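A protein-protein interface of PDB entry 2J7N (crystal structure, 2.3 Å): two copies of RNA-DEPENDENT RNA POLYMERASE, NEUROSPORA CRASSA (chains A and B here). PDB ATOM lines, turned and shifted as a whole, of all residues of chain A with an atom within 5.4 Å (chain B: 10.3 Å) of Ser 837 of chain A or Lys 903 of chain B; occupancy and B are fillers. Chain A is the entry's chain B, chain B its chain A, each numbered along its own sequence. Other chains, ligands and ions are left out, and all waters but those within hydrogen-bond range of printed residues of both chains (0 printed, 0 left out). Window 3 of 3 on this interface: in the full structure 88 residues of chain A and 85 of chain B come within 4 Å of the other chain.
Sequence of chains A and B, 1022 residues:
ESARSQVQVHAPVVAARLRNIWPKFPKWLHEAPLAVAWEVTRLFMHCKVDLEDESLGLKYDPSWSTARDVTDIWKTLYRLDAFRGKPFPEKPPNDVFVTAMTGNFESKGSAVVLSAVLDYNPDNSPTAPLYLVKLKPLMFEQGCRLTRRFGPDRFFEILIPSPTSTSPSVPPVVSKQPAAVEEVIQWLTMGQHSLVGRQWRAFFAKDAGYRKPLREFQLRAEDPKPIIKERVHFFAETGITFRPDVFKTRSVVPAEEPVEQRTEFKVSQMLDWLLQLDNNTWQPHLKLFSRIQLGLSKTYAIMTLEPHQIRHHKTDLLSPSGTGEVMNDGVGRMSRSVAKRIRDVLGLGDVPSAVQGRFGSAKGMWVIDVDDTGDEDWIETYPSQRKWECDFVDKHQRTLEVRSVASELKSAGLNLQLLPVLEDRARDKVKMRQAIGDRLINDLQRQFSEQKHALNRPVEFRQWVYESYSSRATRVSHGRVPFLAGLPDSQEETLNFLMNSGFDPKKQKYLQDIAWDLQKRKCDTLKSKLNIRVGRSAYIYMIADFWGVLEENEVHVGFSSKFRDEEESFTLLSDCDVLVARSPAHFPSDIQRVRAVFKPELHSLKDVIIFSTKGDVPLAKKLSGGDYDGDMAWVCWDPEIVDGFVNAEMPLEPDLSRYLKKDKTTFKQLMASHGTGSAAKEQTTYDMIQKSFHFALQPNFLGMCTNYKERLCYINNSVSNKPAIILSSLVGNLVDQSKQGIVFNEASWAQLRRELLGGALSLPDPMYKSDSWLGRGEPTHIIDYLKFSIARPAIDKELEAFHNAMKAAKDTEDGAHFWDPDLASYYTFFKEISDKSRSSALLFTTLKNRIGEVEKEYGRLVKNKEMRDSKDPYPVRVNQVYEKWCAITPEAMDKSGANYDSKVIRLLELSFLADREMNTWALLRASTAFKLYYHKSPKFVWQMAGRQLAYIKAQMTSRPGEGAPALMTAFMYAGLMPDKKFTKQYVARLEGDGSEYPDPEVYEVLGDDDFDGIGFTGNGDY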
ATOM      1  N   ILE A 833     -15.008  24.702  29.087  1.00  0.00           N
ATOM      2  CA  ILE A 833     -15.786  24.831  27.852  1.00  0.00           C
ATOM      3  C   ILE A 833     -16.447  23.509  27.516  1.00  0.00           C
ATOM      4  O   ILE A 833     -17.611  23.451  27.105  1.00  0.00           O
ATOM      5  CB  ILE A 833     -14.887  25.281  26.681  1.00  0.00           C
ATOM      6  CG1 ILE A 833     -14.757  26.803  26.655  1.00  0.00           C
ATOM      7  CG2 ILE A 833     -15.454  24.804  25.359  1.00  0.00           C
ATOM      8  CD1 ILE A 833     -13.931  27.327  25.502  1.00  0.00           C
ATOM      9  N   SER A 834     -15.631  22.475  27.686  1.00  0.00           N
ATOM     10  CA  SER A 834     -15.982  21.073  27.791  1.00  0.00           C
ATOM     11  C   SER A 834     -16.873  20.682  28.976  1.00  0.00           C
ATOM     12  O   SER A 834     -16.989  19.496  29.278  1.00  0.00           O
ATOM     13  CB  SER A 834     -14.690  20.252  27.889  1.00  0.00           C
ATOM     14  OG  SER A 834     -13.814  20.562  26.823  1.00  0.00           O
ATOM     15  N   ASP A 835     -17.491  21.637  29.661  1.00  0.00           N
ATOM     16  CA  ASP A 835     -18.336  21.249  30.790  1.00  0.00           C
ATOM     17  C   ASP A 835     -19.800  21.344  30.410  1.00  0.00           C
ATOM     18  O   ASP A 835     -20.590  20.421  30.671  1.00  0.00           O
ATOM     19  CB  ASP A 835     -17.981  22.020  32.064  1.00  0.00           C
ATOM     20  CG  ASP A 835     -16.834  21.370  32.830  1.00  0.00           C
ATOM     21  OD1 ASP A 835     -16.330  20.315  32.365  1.00  0.00           O
ATOM     22  OD2 ASP A 835     -16.433  21.907  33.889  1.00  0.00           O
ATOM     23  N   LYS A 836     -20.111  22.493  29.809  1.00  0.00           N
ATOM     24  CA  LYS A 836     -21.177  22.697  28.840  1.00  0.00           C
ATOM     25  C   LYS A 836     -20.696  22.226  27.449  1.00  0.00           C
ATOM     26  O   LYS A 836     -21.064  22.810  26.423  1.00  0.00           O
ATOM     27  CB  LYS A 836     -21.577  24.181  28.765  1.00  0.00           C
ATOM     28  CG  LYS A 836     -21.162  25.054  29.957  1.00  0.00           C
ATOM     29  CD  LYS A 836     -22.001  24.782  31.204  1.00  0.00           C
ATOM     30  CE  LYS A 836     -23.501  24.913  30.941  1.00  0.00           C
ATOM     31  NZ  LYS A 836     -23.964  26.327  30.822  1.00  0.00           N
ATOM     32  N   SER A 837     -19.908  21.145  27.452  1.00  0.00           N
ATOM     33  CA  SER A 837     -19.165  20.570  26.290  1.00  0.00           C
ATOM     34  C   SER A 837     -19.565  20.899  24.836  1.00  0.00           C
ATOM     35  O   SER A 837     -18.981  21.806  24.269  1.00  0.00           O
ATOM     36  CB  SER A 837     -18.951  19.065  26.489  1.00  0.00           C
ATOM     37  OG  SER A 837     -19.883  18.541  27.420  1.00  0.00           O
ATOM     38  N   ARG A 838     -20.460  20.180  24.151  1.00  0.00           N
ATOM     39  CA  ARG A 838     -21.013  18.863  24.403  1.00  0.00           C
ATOM     40  C   ARG A 838     -20.179  17.580  24.111  1.00  0.00           C
ATOM     41  O   ARG A 838     -20.597  16.544  24.609  1.00  0.00           O
ATOM     42  CB  ARG A 838     -22.407  18.744  23.773  1.00  0.00           C
ATOM     43  CG  ARG A 838     -23.461  19.525  24.527  1.00  0.00           C
ATOM     44  CD  ARG A 838     -24.849  19.203  24.029  1.00  0.00           C
ATOM     45  NE  ARG A 838     -25.841  19.345  25.089  1.00  0.00           N
ATOM     46  CZ  ARG A 838     -27.153  19.252  24.901  1.00  0.00           C
ATOM     47  NH1 ARG A 838     -27.637  19.022  23.686  1.00  0.00           N
ATOM     48  NH2 ARG A 838     -27.982  19.388  25.927  1.00  0.00           N
ATOM     49  N   SER A 839     -19.091  17.506  23.328  1.00  0.00           N
ATOM     50  CA  SER A 839     -18.720  18.112  22.052  1.00  0.00           C
ATOM     51  C   SER A 839     -17.229  18.474  22.017  1.00  0.00           C
ATOM     52  O   SER A 839     -16.463  18.001  21.165  1.00  0.00           O
ATOM     53  CB  SER A 839     -19.584  19.312  21.674  1.00  0.00           C
ATOM     54  OG  SER A 839     -19.009  19.958  20.448  1.00  0.00           O
ATOM     55  N   SER A 840     -16.833  19.337  22.943  1.00  0.00           N
ATOM     56  CA  SER A 840     -15.462  19.818  23.001  1.00  0.00           C
ATOM     57  C   SER A 840     -14.747  19.022  24.073  1.00  0.00           C
ATOM     58  O   SER A 840     -13.507  18.929  24.091  1.00  0.00           O
ATOM     59  CB  SER A 840     -15.428  21.320  23.303  1.00  0.00           C
ATOM     60  OG  SER A 840     -16.062  22.062  22.270  1.00  0.00           O
ATOM     61  N   ALA A 841     -15.586  18.516  24.978  1.00  0.00           N
ATOM     62  CA  ALA A 841     -15.399  17.315  25.766  1.00  0.00           C
ATOM     63  C   ALA A 841     -14.774  16.175  24.975  1.00  0.00           C
ATOM     64  O   ALA A 841     -13.698  15.700  25.343  1.00  0.00           O
ATOM     65  CB  ALA A 841     -16.733  16.860  26.354  1.00  0.00           C
ATOM     66  N   VAL A 904     -14.544  25.777  16.492  1.00  0.00           N
ATOM     67  CA  VAL A 904     -13.634  25.673  17.620  1.00  0.00           C
ATOM     68  C   VAL A 904     -12.301  25.061  17.203  1.00  0.00           C
ATOM     69  O   VAL A 904     -11.239  25.514  17.657  1.00  0.00           O
ATOM     70  CB  VAL A 904     -14.269  24.869  18.783  1.00  0.00           C
ATOM     71  CG1 VAL A 904     -13.209  24.254  19.690  1.00  0.00           C
ATOM     72  CG2 VAL A 904     -15.238  25.746  19.580  1.00  0.00           C
ATOM     73  N   PHE B 830     -10.887  35.117   9.588  1.00  0.00           N
ATOM     74  CA  PHE B 830     -12.174  35.333  10.214  1.00  0.00           C
ATOM     75  C   PHE B 830     -13.227  35.821   9.224  1.00  0.00           C
ATOM     76  O   PHE B 830     -14.419  35.778   9.510  1.00  0.00           O
ATOM     77  CB  PHE B 830     -12.051  36.288  11.406  1.00  0.00           C
ATOM     78  CG  PHE B 830     -13.097  36.062  12.457  1.00  0.00           C
ATOM     79  CD1 PHE B 830     -12.960  35.034  13.378  1.00  0.00           C
ATOM     80  CD2 PHE B 830     -14.238  36.857  12.508  1.00  0.00           C
ATOM     81  CE1 PHE B 830     -13.939  34.807  14.344  1.00  0.00           C
ATOM     82  CE2 PHE B 830     -15.216  36.640  13.474  1.00  0.00           C
ATOM     83  CZ  PHE B 830     -15.069  35.613  14.391  1.00  0.00           C
ATOM     84  N   ILE B 833     -14.864  32.855   7.980  1.00  0.00           N
ATOM     85  CA  ILE B 833     -15.587  32.169   9.024  1.00  0.00           C
ATOM     86  C   ILE B 833     -17.058  32.496   9.346  1.00  0.00           C
ATOM     87  O   ILE B 833     -17.848  31.561   9.354  1.00  0.00           O
ATOM     88  CB  ILE B 833     -14.765  32.169  10.354  1.00  0.00           C
ATOM     89  CG1 ILE B 833     -14.968  30.852  11.131  1.00  0.00           C
ATOM     90  CG2 ILE B 833     -15.142  33.374  11.233  1.00  0.00           C
ATOM     91  CD1 ILE B 833     -13.879  30.615  12.209  1.00  0.00           C
ATOM     92  N   SER B 839     -23.317  34.715  12.262  1.00  0.00           N
ATOM     93  CA  SER B 839     -23.408  35.695  13.297  1.00  0.00           C
ATOM     94  C   SER B 839     -21.996  35.965  13.793  1.00  0.00           C
ATOM     95  O   SER B 839     -21.807  36.504  14.880  1.00  0.00           O
ATOM     96  CB  SER B 839     -24.244  35.153  14.455  1.00  0.00           C
ATOM     97  OG  SER B 839     -23.515  34.178  15.189  1.00  0.00           O
ATOM     98  N   SER B 840     -21.004  35.603  12.987  1.00  0.00           N
ATOM     99  CA  SER B 840     -19.645  35.942  13.337  1.00  0.00           C
ATOM    100  C   SER B 840     -18.896  36.962  12.452  1.00  0.00           C
ATOM    101  O   SER B 840     -17.968  37.567  12.964  1.00  0.00           O
ATOM    102  CB  SER B 840     -18.795  34.666  13.477  1.00  0.00           C
ATOM    103  OG  SER B 840     -19.403  33.739  14.456  1.00  0.00           O
ATOM    104  N   LEU B 843     -20.390  39.903  14.626  1.00  0.00           N
ATOM    105  CA  LEU B 843     -19.266  40.272  15.477  1.00  0.00           C
ATOM    106  C   LEU B 843     -18.172  40.958  14.656  1.00  0.00           C
ATOM    107  O   LEU B 843     -17.631  41.987  15.057  1.00  0.00           O
ATOM    108  CB  LEU B 843     -18.695  39.040  16.174  1.00  0.00           C
ATOM    109  CG  LEU B 843     -18.021  39.211  17.539  1.00  0.00           C
ATOM    110  CD1 LEU B 843     -16.814  38.286  17.604  1.00  0.00           C
ATOM    111  CD2 LEU B 843     -17.605  40.657  17.812  1.00  0.00           C
ATOM    112  N   PRO B 890     -14.773  42.323  22.319  1.00  0.00           N
ATOM    113  CA  PRO B 890     -15.859  41.453  21.867  1.00  0.00           C
ATOM    114  C   PRO B 890     -16.988  41.416  22.876  1.00  0.00           C
ATOM    115  O   PRO B 890     -17.846  42.295  22.854  1.00  0.00           O
ATOM    116  CB  PRO B 890     -15.197  40.079  21.767  1.00  0.00           C
ATOM    117  CG  PRO B 890     -14.068  40.133  22.734  1.00  0.00           C
ATOM    118  CD  PRO B 890     -13.617  41.565  22.827  1.00  0.00           C
ATOM    119  N   SER B 902     -20.766  31.985  24.670  1.00  0.00           N
ATOM    120  CA  SER B 902     -20.205  30.940  23.815  1.00  0.00           C
ATOM    121  C   SER B 902     -19.384  31.555  22.708  1.00  0.00           C
ATOM    122  O   SER B 902     -19.426  32.763  22.536  1.00  0.00           O
ATOM    123  CB  SER B 902     -21.319  30.113  23.180  1.00  0.00           C
ATOM    124  OG  SER B 902     -20.932  29.691  21.878  1.00  0.00           O
ATOM    125  N   LYS B 903     -18.559  30.802  21.987  1.00  0.00           N
ATOM    126  CA  LYS B 903     -17.634  29.782  22.424  1.00  0.00           C
ATOM    127  C   LYS B 903     -16.464  30.379  21.640  1.00  0.00           C
ATOM    128  O   LYS B 903     -15.304  30.315  22.038  1.00  0.00           O
ATOM    129  CB  LYS B 903     -18.028  28.441  21.824  1.00  0.00           C
ATOM    130  CG  LYS B 903     -17.532  27.213  22.546  1.00  0.00           C
ATOM    131  CD  LYS B 903     -18.230  25.996  21.961  1.00  0.00           C
ATOM    132  CE  LYS B 903     -18.221  24.826  22.919  1.00  0.00           C
ATOM    133  NZ  LYS B 903     -19.223  23.798  22.521  1.00  0.00           N
ATOM    134  N   VAL B 904     -16.840  31.003  20.523  1.00  0.00           N
ATOM    135  CA  VAL B 904     -15.970  31.751  19.621  1.00  0.00           C
ATOM    136  C   VAL B 904     -15.408  33.015  20.285  1.00  0.00           C
ATOM    137  O   VAL B 904     -14.235  33.353  20.099  1.00  0.00           O
ATOM    138  CB  VAL B 904     -16.751  32.139  18.328  1.00  0.00           C
ATOM    139  CG1 VAL B 904     -16.039  33.228  17.535  1.00  0.00           C
ATOM    140  CG2 VAL B 904     -17.001  30.911  17.461  1.00  0.00           C
ATOM    141  N   ILE B 905     -16.251  33.708  21.053  1.00  0.00           N
ATOM    142  CA  ILE B 905     -15.827  34.909  21.790  1.00  0.00           C
ATOM    143  C   ILE B 905     -14.903  34.541  22.946  1.00  0.00           C
ATOM    144  O   ILE B 905     -13.970  35.279  23.271  1.00  0.00           O
ATOM    145  CB  ILE B 905     -17.027  35.714  22.348  1.00  0.00           C
ATOM    146  CG1 ILE B 905     -17.697  34.964  23.506  1.00  0.00           C
ATOM    147  CG2 ILE B 905     -18.025  36.033  21.243  1.00  0.00           C
ATOM    148  CD1 ILE B 905     -17.250  35.396  24.908  1.00  0.00           C
ATOM    149  N   ARG B 906     -15.164  33.389  23.553  1.00  0.00           N
ATOM    150  CA  ARG B 906     -14.344  32.907  24.643  1.00  0.00           C
ATOM    151  C   ARG B 906     -12.947  32.569  24.172  1.00  0.00           C
ATOM    152  O   ARG B 906     -11.980  32.826  24.876  1.00  0.00           O
ATOM    153  CB  ARG B 906     -14.992  31.706  25.326  1.00  0.00           C
ATOM    154  CG  ARG B 906     -15.900  32.104  26.458  1.00  0.00           C
ATOM    155  CD  ARG B 906     -16.836  30.982  26.806  1.00  0.00           C
ATOM    156  NE  ARG B 906     -16.486  30.316  28.064  1.00  0.00           N
ATOM    157  CZ  ARG B 906     -17.013  29.140  28.426  1.00  0.00           C
ATOM    158  NH1 ARG B 906     -17.892  28.496  27.612  1.00  0.00           N
ATOM    159  NH2 ARG B 906     -16.652  28.601  29.591  1.00  0.00           N
ATOM    160  N   LEU B 907     -12.846  32.002  22.976  1.00  0.00           N
ATOM    161  CA  LEU B 907     -11.552  31.655  22.414  1.00  0.00           C
ATOM    162  C   LEU B 907     -10.776  32.895  21.967  1.00  0.00           C
ATOM    163  O   LEU B 907      -9.565  32.957  22.114  1.00  0.00           O
ATOM    164  CB  LEU B 907     -11.717  30.666  21.257  1.00  0.00           C
ATOM    165  CG  LEU B 907     -11.808  29.206  21.705  1.00  0.00           C
ATOM    166  CD1 LEU B 907     -12.616  28.357  20.715  1.00  0.00           C
ATOM    167  CD2 LEU B 907     -10.396  28.648  21.937  1.00  0.00           C
ATOM    168  N   LEU B 908     -11.489  33.880  21.431  1.00  0.00           N
ATOM    169  CA  LEU B 908     -10.872  35.139  21.034  1.00  0.00           C
ATOM    170  C   LEU B 908     -10.449  35.958  22.254  1.00  0.00           C
ATOM    171  O   LEU B 908      -9.450  36.661  22.220  1.00  0.00           O
ATOM    172  CB  LEU B 908     -11.856  35.960  20.197  1.00  0.00           C
ATOM    173  CG  LEU B 908     -12.229  35.461  18.803  1.00  0.00           C
ATOM    174  CD1 LEU B 908     -13.512  36.138  18.306  1.00  0.00           C
ATOM    175  CD2 LEU B 908     -11.073  35.706  17.845  1.00  0.00           C
ATOM    176  N   GLU B 909     -11.226  35.858  23.325  1.00  0.00           N
ATOM    177  CA  GLU B 909     -11.049  36.699  24.504  1.00  0.00           C
ATOM    178  C   GLU B 909      -9.993  36.180  25.498  1.00  0.00           C
ATOM    179  O   GLU B 909      -9.328  36.982  26.144  1.00  0.00           O
ATOM    180  CB  GLU B 909     -12.408  36.882  25.204  1.00  0.00           C
ATOM    181  CG  GLU B 909     -12.780  38.323  25.529  1.00  0.00           C
ATOM    182  CD  GLU B 909     -14.056  38.421  26.375  1.00  0.00           C
ATOM    183  OE1 GLU B 909     -14.164  37.713  27.405  1.00  0.00           O
ATOM    184  OE2 GLU B 909     -14.960  39.209  26.016  1.00  0.00           O
ATOM    185  N   LEU B 910      -9.853  34.857  25.620  1.00  0.00           N
ATOM    186  CA  LEU B 910      -8.916  34.246  26.581  1.00  0.00           C
ATOM    187  C   LEU B 910      -8.810  35.062  27.883  1.00  0.00           C
ATOM    188  O   LEU B 910      -7.748  35.630  28.188  1.00  0.00           O
ATOM    189  CB  LEU B 910      -7.508  34.070  25.967  1.00  0.00           C
ATOM    190  CG  LEU B 910      -7.254  33.328  24.642  1.00  0.00           C
ATOM    191  CD1 LEU B 910      -5.773  33.489  24.186  1.00  0.00           C
ATOM    192  CD2 LEU B 910      -7.638  31.857  24.711  1.00  0.00           C
ATOM    193  N   SER B 911      -9.907  35.122  28.637  1.00  0.00           N
ATOM    194  CA  SER B 911     -10.031  36.044  29.765  1.00  0.00           C
ATOM    195  C   SER B 911      -9.178  35.670  30.965  1.00  0.00           C
ATOM    196  O   SER B 911      -9.008  36.467  31.888  1.00  0.00           O
ATOM    197  CB  SER B 911     -11.492  36.172  30.200  1.00  0.00           C
ATOM    198  OG  SER B 911     -12.213  36.967  29.276  1.00  0.00           O
ATOM    199  N   PHE B 912      -8.677  34.441  30.967  1.00  0.00           N
ATOM    200  CA  PHE B 912      -7.749  33.992  32.006  1.00  0.00           C
ATOM    201  C   PHE B 912      -6.392  34.736  31.905  1.00  0.00           C
ATOM    202  O   PHE B 912      -5.572  34.663  32.811  1.00  0.00           O
ATOM    203  CB  PHE B 912      -7.567  32.471  31.939  1.00  0.00           C
ATOM    204  CG  PHE B 912      -7.068  31.981  30.602  1.00  0.00           C
ATOM    205  CD1 PHE B 912      -5.708  31.947  30.330  1.00  0.00           C
ATOM    206  CD2 PHE B 912      -7.964  31.556  29.615  1.00  0.00           C
ATOM    207  CE1 PHE B 912      -5.239  31.502  29.103  1.00  0.00           C
ATOM    208  CE2 PHE B 912      -7.500  31.112  28.385  1.00  0.00           C
ATOM    209  CZ  PHE B 912      -6.127  31.086  28.134  1.00  0.00           C
ATOM    210  N   THR B 920      -6.162  36.512  21.423  1.00  0.00           N
ATOM    211  CA  THR B 920      -6.295  36.275  19.985  1.00  0.00           C
ATOM    212  C   THR B 920      -7.139  37.367  19.322  1.00  0.00           C
ATOM    213  O   THR B 920      -6.965  37.667  18.133  1.00  0.00           O
ATOM    214  CB  THR B 920      -6.927  34.914  19.738  1.00  0.00           C
ATOM    215  OG1 THR B 920      -6.301  33.956  20.606  1.00  0.00           O
ATOM    216  CG2 THR B 920      -6.761  34.509  18.295  1.00  0.00           C
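The side-chain amino group of Lys 903 of chain B sits at hydrogen-bond distance from the backbone carbonyl oxygen of Ser 837 of chain A (2.7 Å).
The side-chain hydroxyl (OG) of Ser 834 of chain A lies within hydrogen-bond range of the backbone carbonyl oxygen (O) of Ser 840 of chain A (3.2 Å).
Ile 833 of chain A touches Lys 903 of chain B. Ile 833 of chain A touches Arg 906 of chain B (CG1 to NH1, 3.7 Å). OG of Ser 840 of chain A touches CE of Lys 903 of chain B, at 3.6 Å. Val 904 of chain A touches Lys 903 of chain B. Val 904 of chain A touches Leu 907 of chain B.
Asp 835 of chain A touches none of the printed residues of chain B. Ser 837 of chain A touches just one residue of chain B: Lys 903. Printed residues of chain B within 4 Å of Val 904 of chain A: Lys 903 and Leu 907. Of the printed residues of chain A, Leu 907 of chain B touches Val 904 (3.9 Å). The nearest residue of chain A that does not touch Lys 903 of chain B is Arg 838 of chain A (4.2 Å). The nearest printed residue of chain B that does not touch Ile 833 of chain A is Leu 907 of chain B (4.7 Å).
Of the 18 printed residues of chain B, 3 touch a printed residue of chain A. Printed residues of chain B that touch a printed residue of chain A: Lys 903, Arg 906 and Leu 907. Of the 10 printed residues of chain A, 4 touch a printed residue of chain B. Among the printed residues, no Asp or Glu carboxylate lies within 4 Å of a Lys or Arg side-chain nitrogen of the other chain.
Positions printed for both chains: 833, 839, 840 and 904. Of the 6 pairs that touch across the chains among the printed residues, none has its exchanged pair printed and touching as well.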
